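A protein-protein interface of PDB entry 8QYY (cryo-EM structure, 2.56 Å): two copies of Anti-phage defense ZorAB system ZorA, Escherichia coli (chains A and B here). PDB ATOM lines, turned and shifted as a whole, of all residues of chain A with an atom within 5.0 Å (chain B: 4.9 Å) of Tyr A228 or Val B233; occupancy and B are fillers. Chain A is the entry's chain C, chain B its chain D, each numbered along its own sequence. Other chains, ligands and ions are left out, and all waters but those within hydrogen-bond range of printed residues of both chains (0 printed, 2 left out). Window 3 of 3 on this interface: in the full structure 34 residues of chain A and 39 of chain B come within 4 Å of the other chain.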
ATOM      1  N   HIS A  92      18.501  -5.292 -30.702  1.00  0.00           N
ATOM      2  CA  HIS A  92      17.112  -5.627 -30.989  1.00  0.00           C
ATOM      3  C   HIS A  92      16.661  -4.839 -32.210  1.00  0.00           C
ATOM      4  O   HIS A  92      16.608  -3.606 -32.175  1.00  0.00           O
ATOM      5  CB  HIS A  92      16.217  -5.328 -29.791  1.00  0.00           C
ATOM      6  CG  HIS A  92      14.771  -5.607 -30.043  1.00  0.00           C
ATOM      7  ND1 HIS A  92      14.273  -6.885 -30.167  1.00  0.00           N
ATOM      8  CD2 HIS A  92      13.721  -4.774 -30.219  1.00  0.00           C
ATOM      9  CE1 HIS A  92      12.976  -6.827 -30.398  1.00  0.00           C
ATOM     10  NE2 HIS A  92      12.614  -5.558 -30.433  1.00  0.00           N
ATOM     11  N   GLN A  94      13.754  -3.716 -34.733  1.00  0.00           N
ATOM     12  CA  GLN A  94      12.309  -3.537 -34.738  1.00  0.00           C
ATOM     13  C   GLN A  94      11.810  -3.574 -36.174  1.00  0.00           C
ATOM     14  O   GLN A  94      12.238  -2.769 -37.005  1.00  0.00           O
ATOM     15  CB  GLN A  94      11.919  -2.224 -34.064  1.00  0.00           C
ATOM     16  CG  GLN A  94      12.513  -2.052 -32.682  1.00  0.00           C
ATOM     17  CD  GLN A  94      11.907  -0.892 -31.931  1.00  0.00           C
ATOM     18  OE1 GLN A  94      12.066   0.262 -32.318  1.00  0.00           O
ATOM     19  NE2 GLN A  94      11.213  -1.190 -30.844  1.00  0.00           N
ATOM     20  N   VAL A 224      14.087  -0.228 -24.786  1.00  0.00           N
ATOM     21  CA  VAL A 224      13.050  -0.801 -25.637  1.00  0.00           C
ATOM     22  C   VAL A 224      12.074  -1.650 -24.825  1.00  0.00           C
ATOM     23  O   VAL A 224      10.877  -1.686 -25.130  1.00  0.00           O
ATOM     24  CB  VAL A 224      13.691  -1.595 -26.792  1.00  0.00           C
ATOM     25  CG1 VAL A 224      14.454  -2.805 -26.279  1.00  0.00           C
ATOM     26  CG2 VAL A 224      12.644  -1.998 -27.807  1.00  0.00           C
ATOM     27  N   GLY A 225      12.552  -2.338 -23.785  1.00  0.00           N
ATOM     28  CA  GLY A 225      11.666  -3.182 -23.001  1.00  0.00           C
ATOM     29  C   GLY A 225      10.624  -2.394 -22.229  1.00  0.00           C
ATOM     30  O   GLY A 225       9.458  -2.796 -22.151  1.00  0.00           O
ATOM     31  N   GLU A 226      11.030  -1.269 -21.641  1.00  0.00           N
ATOM     32  CA  GLU A 226      10.076  -0.412 -20.946  1.00  0.00           C
ATOM     33  C   GLU A 226       9.044   0.151 -21.912  1.00  0.00           C
ATOM     34  O   GLU A 226       7.862   0.262 -21.573  1.00  0.00           O
ATOM     35  CB  GLU A 226      10.813   0.714 -20.226  1.00  0.00           C
ATOM     36  CG  GLU A 226      11.406   0.309 -18.890  1.00  0.00           C
ATOM     37  CD  GLU A 226      12.778  -0.324 -19.027  1.00  0.00           C
ATOM     38  OE1 GLU A 226      13.316  -0.352 -20.153  1.00  0.00           O
ATOM     39  OE2 GLU A 226      13.322  -0.791 -18.005  1.00  0.00           O
ATOM     40  N   GLU A 227       9.474   0.516 -23.122  1.00  0.00           N
ATOM     41  CA  GLU A 227       8.533   0.988 -24.132  1.00  0.00           C
ATOM     42  C   GLU A 227       7.547  -0.105 -24.520  1.00  0.00           C
ATOM     43  O   GLU A 227       6.355   0.162 -24.703  1.00  0.00           O
ATOM     44  CB  GLU A 227       9.289   1.488 -25.358  1.00  0.00           C
ATOM     45  CG  GLU A 227      10.149   2.703 -25.094  1.00  0.00           C
ATOM     46  CD  GLU A 227      10.899   3.158 -26.321  1.00  0.00           C
ATOM     47  OE1 GLU A 227      10.705   2.550 -27.394  1.00  0.00           O
ATOM     48  OE2 GLU A 227      11.683   4.125 -26.217  1.00  0.00           O
ATOM     49  N   TYR A 228       8.028  -1.342 -24.652  1.00  0.00           N
ATOM     50  CA  TYR A 228       7.134  -2.451 -24.963  1.00  0.00           C
ATOM     51  C   TYR A 228       6.118  -2.671 -23.851  1.00  0.00           C
ATOM     52  O   TYR A 228       4.934  -2.902 -24.119  1.00  0.00           O
ATOM     53  CB  TYR A 228       7.943  -3.725 -25.201  1.00  0.00           C
ATOM     54  CG  TYR A 228       8.603  -3.796 -26.554  1.00  0.00           C
ATOM     55  CD1 TYR A 228       8.079  -3.114 -27.638  1.00  0.00           C
ATOM     56  CD2 TYR A 228       9.746  -4.555 -26.747  1.00  0.00           C
ATOM     57  CE1 TYR A 228       8.677  -3.181 -28.872  1.00  0.00           C
ATOM     58  CE2 TYR A 228      10.349  -4.630 -27.977  1.00  0.00           C
ATOM     59  CZ  TYR A 228       9.812  -3.940 -29.038  1.00  0.00           C
ATOM     60  OH  TYR A 228      10.409  -4.009 -30.272  1.00  0.00           O
ATOM     61  N   LEU A 229       6.560  -2.610 -22.595  1.00  0.00           N
ATOM     62  CA  LEU A 229       5.632  -2.785 -21.482  1.00  0.00           C
ATOM     63  C   LEU A 229       4.610  -1.654 -21.425  1.00  0.00           C
ATOM     64  O   LEU A 229       3.432  -1.889 -21.129  1.00  0.00           O
ATOM     65  CB  LEU A 229       6.395  -2.888 -20.164  1.00  0.00           C
ATOM     66  CG  LEU A 229       6.999  -4.253 -19.836  1.00  0.00           C
ATOM     67  CD1 LEU A 229       7.426  -4.294 -18.386  1.00  0.00           C
ATOM     68  CD2 LEU A 229       6.016  -5.364 -20.133  1.00  0.00           C
ATOM     69  N   ALA A 230       5.041  -0.421 -21.696  1.00  0.00           N
ATOM     70  CA  ALA A 230       4.105   0.698 -21.736  1.00  0.00           C
ATOM     71  C   ALA A 230       3.081   0.517 -22.848  1.00  0.00           C
ATOM     72  O   ALA A 230       1.889   0.792 -22.659  1.00  0.00           O
ATOM     73  CB  ALA A 230       4.866   2.009 -21.917  1.00  0.00           C
ATOM     74  N   SER A 231       3.531   0.050 -24.014  1.00  0.00           N
ATOM     75  CA  SER A 231       2.610  -0.247 -25.102  1.00  0.00           C
ATOM     76  C   SER A 231       1.618  -1.328 -24.701  1.00  0.00           C
ATOM     77  O   SER A 231       0.434  -1.246 -25.034  1.00  0.00           O
ATOM     78  CB  SER A 231       3.387  -0.675 -26.344  1.00  0.00           C
ATOM     79  OG  SER A 231       3.910   0.447 -27.029  1.00  0.00           O
ATOM     80  N   LEU A 232       2.085  -2.354 -23.991  1.00  0.00           N
ATOM     81  CA  LEU A 232       1.192  -3.427 -23.564  1.00  0.00           C
ATOM     82  C   LEU A 232       0.143  -2.922 -22.581  1.00  0.00           C
ATOM     83  O   LEU A 232      -1.029  -3.302 -22.669  1.00  0.00           O
ATOM     84  CB  LEU A 232       2.002  -4.566 -22.948  1.00  0.00           C
ATOM     85  CG  LEU A 232       2.782  -5.426 -23.940  1.00  0.00           C
ATOM     86  CD1 LEU A 232       3.696  -6.376 -23.203  1.00  0.00           C
ATOM     87  CD2 LEU A 232       1.828  -6.186 -24.831  1.00  0.00           C
ATOM     88  N   GLU B 226      13.333  -9.599 -25.549  1.00  0.00           N
ATOM     89  CA  GLU B 226      12.867  -8.460 -26.328  1.00  0.00           C
ATOM     90  C   GLU B 226      12.043  -8.910 -27.525  1.00  0.00           C
ATOM     91  O   GLU B 226      11.060  -8.258 -27.886  1.00  0.00           O
ATOM     92  CB  GLU B 226      14.049  -7.604 -26.776  1.00  0.00           C
ATOM     93  CG  GLU B 226      14.480  -6.566 -25.759  1.00  0.00           C
ATOM     94  CD  GLU B 226      15.369  -7.139 -24.674  1.00  0.00           C
ATOM     95  OE1 GLU B 226      15.825  -8.292 -24.818  1.00  0.00           O
ATOM     96  OE2 GLU B 226      15.617  -6.432 -23.675  1.00  0.00           O
ATOM     97  N   LEU B 229       8.632  -9.742 -26.155  1.00  0.00           N
ATOM     98  CA  LEU B 229       7.880  -8.526 -25.862  1.00  0.00           C
ATOM     99  C   LEU B 229       7.374  -7.862 -27.138  1.00  0.00           C
ATOM    100  O   LEU B 229       6.240  -7.370 -27.188  1.00  0.00           O
ATOM    101  CB  LEU B 229       8.746  -7.557 -25.060  1.00  0.00           C
ATOM    102  CG  LEU B 229       8.935  -7.865 -23.577  1.00  0.00           C
ATOM    103  CD1 LEU B 229       9.517  -6.668 -22.862  1.00  0.00           C
ATOM    104  CD2 LEU B 229       7.622  -8.275 -22.947  1.00  0.00           C
ATOM    105  N   ALA B 230       8.206  -7.832 -28.181  1.00  0.00           N
ATOM    106  CA  ALA B 230       7.779  -7.272 -29.457  1.00  0.00           C
ATOM    107  C   ALA B 230       6.629  -8.075 -30.051  1.00  0.00           C
ATOM    108  O   ALA B 230       5.677  -7.503 -30.599  1.00  0.00           O
ATOM    109  CB  ALA B 230       8.958  -7.226 -30.425  1.00  0.00           C
ATOM    110  N   SER B 231       6.704  -9.404 -29.954  1.00  0.00           N
ATOM    111  CA  SER B 231       5.611 -10.245 -30.425  1.00  0.00           C
ATOM    112  C   SER B 231       4.336  -9.970 -29.646  1.00  0.00           C
ATOM    113  O   SER B 231       3.247  -9.928 -30.225  1.00  0.00           O
ATOM    114  CB  SER B 231       5.996 -11.718 -30.312  1.00  0.00           C
ATOM    115  OG  SER B 231       7.035 -12.045 -31.213  1.00  0.00           O
ATOM    116  N   LEU B 232       4.450  -9.783 -28.332  1.00  0.00           N
ATOM    117  CA  LEU B 232       3.275  -9.478 -27.522  1.00  0.00           C
ATOM    118  C   LEU B 232       2.651  -8.150 -27.928  1.00  0.00           C
ATOM    119  O   LEU B 232       1.423  -8.027 -27.990  1.00  0.00           O
ATOM    120  CB  LEU B 232       3.648  -9.464 -26.043  1.00  0.00           C
ATOM    121  CG  LEU B 232       3.859 -10.838 -25.418  1.00  0.00           C
ATOM    122  CD1 LEU B 232       4.333 -10.686 -23.995  1.00  0.00           C
ATOM    123  CD2 LEU B 232       2.578 -11.631 -25.477  1.00  0.00           C
ATOM    124  N   VAL B 233       3.481  -7.143 -28.203  1.00  0.00           N
ATOM    125  CA  VAL B 233       2.958  -5.838 -28.609  1.00  0.00           C
ATOM    126  C   VAL B 233       2.240  -5.944 -29.951  1.00  0.00           C
ATOM    127  O   VAL B 233       1.122  -5.429 -30.126  1.00  0.00           O
ATOM    128  CB  VAL B 233       4.092  -4.800 -28.652  1.00  0.00           C
ATOM    129  CG1 VAL B 233       3.599  -3.498 -29.247  1.00  0.00           C
ATOM    130  CG2 VAL B 233       4.641  -4.571 -27.264  1.00  0.00           C
ATOM    131  N   LYS B 234       2.871  -6.614 -30.918  1.00  0.00           N
ATOM    132  CA  LYS B 234       2.229  -6.797 -32.216  1.00  0.00           C
ATOM    133  C   LYS B 234       0.927  -7.570 -32.079  1.00  0.00           C
ATOM    134  O   LYS B 234      -0.066  -7.249 -32.739  1.00  0.00           O
ATOM    135  CB  LYS B 234       3.167  -7.511 -33.189  1.00  0.00           C
ATOM    136  CG  LYS B 234       4.402  -6.728 -33.577  1.00  0.00           C
ATOM    137  CD  LYS B 234       5.254  -7.519 -34.557  1.00  0.00           C
ATOM    138  CE  LYS B 234       6.456  -6.725 -35.035  1.00  0.00           C
ATOM    139  NZ  LYS B 234       7.416  -6.475 -33.933  1.00  0.00           N
ATOM    140  N   SER B 235       0.917  -8.597 -31.228  1.00  0.00           N
ATOM    141  CA  SER B 235      -0.285  -9.395 -31.036  1.00  0.00           C
ATOM    142  C   SER B 235      -1.400  -8.579 -30.402  1.00  0.00           C
ATOM    143  O   SER B 235      -2.567  -8.755 -30.751  1.00  0.00           O
ATOM    144  CB  SER B 235       0.035 -10.622 -30.187  1.00  0.00           C
ATOM    145  OG  SER B 235       0.735 -11.590 -30.945  1.00  0.00           O
ATOM    146  N   SER B 236      -1.067  -7.683 -29.473  1.00  0.00           N
ATOM    147  CA  SER B 236      -2.093  -6.836 -28.871  1.00  0.00           C
ATOM    148  C   SER B 236      -2.709  -5.895 -29.903  1.00  0.00           C
ATOM    149  O   SER B 236      -3.941  -5.755 -29.983  1.00  0.00           O
ATOM    150  CB  SER B 236      -1.500  -6.043 -27.708  1.00  0.00           C
ATOM    151  OG  SER B 236      -1.075  -6.910 -26.674  1.00  0.00           O
ATOM    152  N   ASN B 237      -1.867  -5.239 -30.703  1.00  0.00           N
ATOM    153  CA  ASN B 237      -2.398  -4.343 -31.730  1.00  0.00           C
ATOM    154  C   ASN B 237      -3.251  -5.111 -32.736  1.00  0.00           C
ATOM    155  O   ASN B 237      -4.365  -4.689 -33.092  1.00  0.00           O
ATOM    156  CB  ASN B 237      -1.250  -3.616 -32.429  1.00  0.00           C
ATOM    157  CG  ASN B 237      -0.368  -2.853 -31.462  1.00  0.00           C
ATOM    158  OD1 ASN B 237      -0.809  -2.452 -30.387  1.00  0.00           O
ATOM    159  ND2 ASN B 237       0.884  -2.648 -31.842  1.00  0.00           N
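Of chain B, only Glu B226, Leu B229, Ala B230 and Val B233 come within 4 Å of Tyr A228. Val B233 touches just these residues of chain A: Tyr A228 and Leu A232. Printed residues of chain A within 4 Å of Glu B226: His A92, Val A224 and Tyr A228. Of the printed residues of chain A, Leu B232 touches Leu A232 (3.7 Å). Leu A229 touches none of the printed residues of chain B. Gln A94 touches none of the printed residues of chain B. The nearest printed residue of chain B that does not touch Tyr A228 is Lys B234 (5.3 Å). The nearest residue of chain A that does not touch Val B233 is Ser A231 (4.1 Å). The nearest printed residue of chain B that does not touch Gly A225 is Glu B226 (5.0 Å).
CE1 of His A92 touches O of Glu B226, 3.5 Å away. Val A224 touches Glu B226 (CG1 to CG, 3.8 Å). Gly A225 touches Leu B229 (O to CD1, 3.9 Å). Glu B226 touches Tyr A228 (O to CE2, 3.7 Å). Tyr A228 touches Leu B229. OH of Tyr A228 touches CB of Ala B230 (3.5 Å). O of Tyr A228 touches CG2 of Val B233, at 3.6 Å. O of Leu B232 touches CD2 of Leu A232, 3.7 Å away. Leu A232 touches Val B233. Leu A232 touches Ser B236.
The side-chain hydroxyl (OG) of Ser B236 is in hydrogen-bond range of the backbone carbonyl oxygen (O) of Leu B232, 3.0 Å away. A ring nitrogen (NE2) of His A92 is in hydrogen-bond range of the side-chain hydroxyl of Tyr A228. The backbone carbonyl oxygen (O) of Val B233 lies close to the side-chain amide nitrogen (ND2) of Asn B237 (3.3 Å). OH of Tyr A228 is in hydrogen-bond range of NE2 of Gln A94.
Printed residues of chain A that touch a printed residue of chain B: His A92, Val A224, Gly A225, Tyr A228 and Leu A232. Hydrophobic or aromatic side chains of chain A within 4 Å of the printed part of chain B: His A92, Val A224, Tyr A228 and Leu A232. Of the 10 printed residues of chain B, 6 touch a printed residue of chain A. Hydrophobic or aromatic side chains of chain B within 4 Å of the printed part of chain A: Leu B229, Ala B230, Leu B232 and Val B233. Among the printed residues, 10 pairs touch across the chains. Among the printed residues, no Asp or Glu carboxylate lies within 4 Å of a Lys or Arg side-chain nitrogen of the other chain.
Leu A232 touches its own counterpart, Leu B232.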
